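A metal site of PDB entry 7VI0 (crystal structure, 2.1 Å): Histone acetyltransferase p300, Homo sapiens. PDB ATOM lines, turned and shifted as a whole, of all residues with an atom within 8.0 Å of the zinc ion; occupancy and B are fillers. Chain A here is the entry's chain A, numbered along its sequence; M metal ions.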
ATOM      1  N   TYR A   6     -11.774   2.974   9.130  1.00  0.00           N
ATOM      2  CA  TYR A   6     -12.761   4.030   9.332  1.00  0.00           C
ATOM      3  C   TYR A   6     -12.200   5.370   8.890  1.00  0.00           C
ATOM      4  O   TYR A   6     -11.026   5.662   9.121  1.00  0.00           O
ATOM      5  CB  TYR A   6     -13.203   4.078  10.789  1.00  0.00           C
ATOM      6  N   CYS A   7     -13.042   6.189   8.248  1.00  0.00           N
ATOM      7  CA  CYS A   7     -12.603   7.463   7.676  1.00  0.00           C
ATOM      8  C   CYS A   7     -11.959   8.336   8.739  1.00  0.00           C
ATOM      9  O   CYS A   7     -10.752   8.585   8.699  1.00  0.00           O
ATOM     10  CB  CYS A   7     -13.796   8.182   7.043  1.00  0.00           C
ATOM     11  SG  CYS A   7     -15.296   8.073   8.052  1.00  0.00           S
ATOM     12  N   CYS A   8     -12.765   8.785   9.698  1.00  0.00           N
ATOM     13  CA  CYS A   8     -12.200   9.274  10.947  1.00  0.00           C
ATOM     14  C   CYS A   8     -11.724   8.082  11.779  1.00  0.00           C
ATOM     15  O   CYS A   8     -12.096   6.931  11.526  1.00  0.00           O
ATOM     16  CB  CYS A   8     -13.250  10.074  11.707  1.00  0.00           C
ATOM     17  SG  CYS A   8     -14.828   9.210  11.814  1.00  0.00           S
ATOM     18  N   GLY A   9     -10.938   8.369  12.808  1.00  0.00           N
ATOM     19  CA  GLY A   9     -10.417   7.319  13.653  1.00  0.00           C
ATOM     20  C   GLY A   9     -11.392   6.944  14.753  1.00  0.00           C
ATOM     21  O   GLY A   9     -10.983   6.459  15.819  1.00  0.00           O
ATOM     22  N   ARG A  10     -12.678   7.149  14.507  1.00  0.00           N
ATOM     23  CA  ARG A  10     -13.687   7.193  15.557  1.00  0.00           C
ATOM     24  C   ARG A  10     -14.646   6.025  15.463  1.00  0.00           C
ATOM     25  O   ARG A  10     -15.135   5.690  14.377  1.00  0.00           O
ATOM     26  CB  ARG A  10     -14.468   8.514  15.488  1.00  0.00           C
ATOM     27  N   LYS A  11     -14.933   5.413  16.613  1.00  0.00           N
ATOM     28  CA  LYS A  11     -15.971   4.392  16.735  1.00  0.00           C
ATOM     29  C   LYS A  11     -17.267   5.094  17.143  1.00  0.00           C
ATOM     30  O   LYS A  11     -17.365   5.615  18.258  1.00  0.00           O
ATOM     31  CB  LYS A  11     -15.572   3.321  17.745  1.00  0.00           C
ATOM     32  CG  LYS A  11     -16.369   2.022  17.623  1.00  0.00           C
ATOM     33  CD  LYS A  11     -16.735   1.457  18.994  1.00  0.00           C
ATOM     34  CE  LYS A  11     -17.463   0.123  18.860  1.00  0.00           C
ATOM     35  NZ  LYS A  11     -18.303  -0.192  20.053  1.00  0.00           N
ATOM     36  N   LEU A  12     -18.247   5.089  16.256  1.00  0.00           N
ATOM     37  CA  LEU A  12     -19.442   5.910  16.402  1.00  0.00           C
ATOM     38  C   LEU A  12     -20.692   5.052  16.421  1.00  0.00           C
ATOM     39  O   LEU A  12     -20.813   4.096  15.655  1.00  0.00           O
ATOM     40  CB  LEU A  12     -19.533   6.942  15.272  1.00  0.00           C
ATOM     41  CG  LEU A  12     -18.417   7.988  15.260  1.00  0.00           C
ATOM     42  CD1 LEU A  12     -18.445   8.790  13.966  1.00  0.00           C
ATOM     43  CD2 LEU A  12     -18.516   8.898  16.471  1.00  0.00           C
ATOM     44  N   GLU A  86     -23.203   3.188  13.683  1.00  0.00           N
ATOM     45  CA  GLU A  86     -23.398   3.969  12.473  1.00  0.00           C
ATOM     46  C   GLU A  86     -23.117   3.102  11.256  1.00  0.00           C
ATOM     47  O   GLU A  86     -22.358   2.133  11.302  1.00  0.00           O
ATOM     48  CB  GLU A  86     -22.483   5.195  12.477  1.00  0.00           C
ATOM     49  CG  GLU A  86     -23.015   6.364  13.307  1.00  0.00           C
ATOM     50  CD  GLU A  86     -22.374   7.683  12.939  1.00  0.00           C
ATOM     51  OE1 GLU A  86     -21.867   7.814  11.798  1.00  0.00           O
ATOM     52  OE2 GLU A  86     -22.376   8.595  13.786  1.00  0.00           O
ATOM     53  N   LEU A  87     -23.750   3.466  10.141  1.00  0.00           N
ATOM     54  CA  LEU A  87     -23.605   2.693   8.914  1.00  0.00           C
ATOM     55  C   LEU A  87     -22.403   3.170   8.124  1.00  0.00           C
ATOM     56  O   LEU A  87     -22.007   4.341   8.189  1.00  0.00           O
ATOM     57  CB  LEU A  87     -24.878   2.805   8.064  1.00  0.00           C
ATOM     58  CG  LEU A  87     -26.189   2.370   8.710  1.00  0.00           C
ATOM     59  CD1 LEU A  87     -27.256   2.110   7.663  1.00  0.00           C
ATOM     60  CD2 LEU A  87     -25.984   1.143   9.590  1.00  0.00           C
ATOM     61  N   PHE A  88     -21.809   2.254   7.372  1.00  0.00           N
ATOM     62  CA  PHE A  88     -20.711   2.544   6.469  1.00  0.00           C
ATOM     63  C   PHE A  88     -21.176   2.437   5.030  1.00  0.00           C
ATOM     64  O   PHE A  88     -22.116   1.708   4.708  1.00  0.00           O
ATOM     65  CB  PHE A  88     -19.537   1.590   6.693  1.00  0.00           C
ATOM     66  CG  PHE A  88     -18.857   1.755   8.027  1.00  0.00           C
ATOM     67  CD1 PHE A  88     -19.456   1.275   9.183  1.00  0.00           C
ATOM     68  CD2 PHE A  88     -17.632   2.388   8.123  1.00  0.00           C
ATOM     69  CE1 PHE A  88     -18.834   1.426  10.412  1.00  0.00           C
ATOM     70  CE2 PHE A  88     -17.009   2.539   9.352  1.00  0.00           C
ATOM     71  CZ  PHE A  88     -17.615   2.048  10.497  1.00  0.00           C
ATOM     72  N   LYS A  97     -14.053   2.064   3.124  1.00  0.00           N
ATOM     73  CA  LYS A  97     -15.262   2.116   3.930  1.00  0.00           C
ATOM     74  C   LYS A  97     -15.259   3.396   4.739  1.00  0.00           C
ATOM     75  O   LYS A  97     -14.282   3.686   5.438  1.00  0.00           O
ATOM     76  CB  LYS A  97     -15.368   0.896   4.849  1.00  0.00           C
ATOM     77  CG  LYS A  97     -16.157  -0.266   4.244  1.00  0.00           C
ATOM     78  CD  LYS A  97     -16.269  -1.425   5.236  1.00  0.00           C
ATOM     79  CE  LYS A  97     -16.182  -2.772   4.536  1.00  0.00           C
ATOM     80  NZ  LYS A  97     -15.434  -3.775   5.336  1.00  0.00           N
ATOM     81  N   MET A  98     -16.332   4.174   4.634  1.00  0.00           N
ATOM     82  CA  MET A  98     -16.484   5.407   5.374  1.00  0.00           C
ATOM     83  C   MET A  98     -17.855   5.453   6.037  1.00  0.00           C
ATOM     84  O   MET A  98     -18.816   4.877   5.521  1.00  0.00           O
ATOM     85  CB  MET A  98     -16.340   6.649   4.466  1.00  0.00           C
ATOM     86  CG  MET A  98     -15.512   6.428   3.218  1.00  0.00           C
ATOM     87  SD  MET A  98     -13.803   6.927   3.456  1.00  0.00           S
ATOM     88  CE  MET A  98     -13.873   8.646   2.972  1.00  0.00           C
ATOM     89  N   HIS A  99     -17.934   6.129   7.175  1.00  0.00           N
ATOM     90  CA  HIS A  99     -19.229   6.443   7.756  1.00  0.00           C
ATOM     91  C   HIS A  99     -20.077   7.160   6.721  1.00  0.00           C
ATOM     92  O   HIS A  99     -19.619   8.099   6.083  1.00  0.00           O
ATOM     93  CB  HIS A  99     -19.060   7.318   8.993  1.00  0.00           C
ATOM     94  CG  HIS A  99     -18.406   6.638  10.157  1.00  0.00           C
ATOM     95  ND1 HIS A  99     -17.225   7.092  10.719  1.00  0.00           N
ATOM     96  CD2 HIS A  99     -18.773   5.556  10.873  1.00  0.00           C
ATOM     97  CE1 HIS A  99     -16.897   6.307  11.730  1.00  0.00           C
ATOM     98  NE2 HIS A  99     -17.819   5.363  11.849  1.00  0.00           N
ATOM     99  N   GLN A 100     -21.312   6.687   6.552  1.00  0.00           N
ATOM    100  CA  GLN A 100     -22.209   7.337   5.596  1.00  0.00           C
ATOM    101  C   GLN A 100     -22.434   8.798   5.959  1.00  0.00           C
ATOM    102  O   GLN A 100     -22.494   9.666   5.083  1.00  0.00           O
ATOM    103  CB  GLN A 100     -23.548   6.590   5.532  1.00  0.00           C
ATOM    104  CG  GLN A 100     -24.453   7.051   4.400  1.00  0.00           C
ATOM    105  CD  GLN A 100     -25.706   6.202   4.277  1.00  0.00           C
ATOM    106  OE1 GLN A 100     -26.076   5.475   5.190  1.00  0.00           O
ATOM    107  NE2 GLN A 100     -26.373   6.308   3.128  1.00  0.00           N
ATOM    108  N   ILE A 101     -22.531   9.095   7.262  1.00  0.00           N
ATOM    109  CA  ILE A 101     -22.761  10.457   7.705  1.00  0.00           C
ATOM    110  C   ILE A 101     -21.549  11.337   7.432  1.00  0.00           C
ATOM    111  O   ILE A 101     -21.679  12.514   7.093  1.00  0.00           O
ATOM    112  CB  ILE A 101     -23.133  10.449   9.207  1.00  0.00           C
ATOM    113  CG1 ILE A 101     -24.480   9.743   9.402  1.00  0.00           C
ATOM    114  CG2 ILE A 101     -23.181  11.863   9.761  1.00  0.00           C
ATOM    115  CD1 ILE A 101     -24.896   9.598  10.858  1.00  0.00           C
ATOM    116  N   CYS A 102     -20.337  10.770   7.552  1.00  0.00           N
ATOM    117  CA  CYS A 102     -19.124  11.563   7.369  1.00  0.00           C
ATOM    118  C   CYS A 102     -18.989  12.075   5.935  1.00  0.00           C
ATOM    119  O   CYS A 102     -18.587  13.213   5.716  1.00  0.00           O
ATOM    120  CB  CYS A 102     -17.897  10.745   7.762  1.00  0.00           C
ATOM    121  SG  CYS A 102     -17.544  10.724   9.526  1.00  0.00           S
ATOM    122  N   VAL A 103     -19.323  11.235   4.956  1.00  0.00           N
ATOM    123  CA  VAL A 103     -19.187  11.611   3.555  1.00  0.00           C
ATOM    124  C   VAL A 103     -20.498  12.084   2.943  1.00  0.00           C
ATOM    125  O   VAL A 103     -20.511  12.502   1.783  1.00  0.00           O
ATOM    126  CB  VAL A 103     -18.600  10.450   2.722  1.00  0.00           C
ATOM    127  CG1 VAL A 103     -17.175  10.167   3.150  1.00  0.00           C
ATOM    128  CG2 VAL A 103     -19.459   9.203   2.860  1.00  0.00           C
ATOM    129  N   ARG A 433     -22.156  17.107  12.315  1.00  0.00           N
ATOM    130  CA  ARG A 433     -22.135  16.129  11.239  1.00  0.00           C
ATOM    131  C   ARG A 433     -23.458  15.375  11.129  1.00  0.00           C
ATOM    132  O   ARG A 433     -23.952  15.158  10.020  1.00  0.00           O
ATOM    133  CB  ARG A 433     -20.968  15.158  11.421  1.00  0.00           C
ATOM    134  CG  ARG A 433     -20.888  14.454  12.771  1.00  0.00           C
ATOM    135  CD  ARG A 433     -19.669  13.558  12.862  1.00  0.00           C
ATOM    136  NE  ARG A 433     -19.671  12.501  11.855  1.00  0.00           N
ATOM    137  CZ  ARG A 433     -20.333  11.355  11.971  1.00  0.00           C
ATOM    138  NH1 ARG A 433     -21.076  11.090  13.039  1.00  0.00           N
ATOM    139  NH2 ARG A 433     -20.255  10.463  10.997  1.00  0.00           N
HETATM  140 ZN    ZN M   1     -16.254   8.846  10.021  1.00  0.00          ZN
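SG of Cys 102 sits close to NH2 of Arg 433 (3.1 Å).
The zinc ion is bound by a ring nitrogen (ND1) of His 99 (2.1 Å), the side-chain sulfur of Cys 8 (2.3 Å), the side-chain sulfur of Cys 7 (2.3 Å) and the side-chain sulfur of Cys 102 (2.3 Å).
Four residues have an atom within 4 Å of the zinc ion: Cys 7, Cys 8, His 99 and Cys 102.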
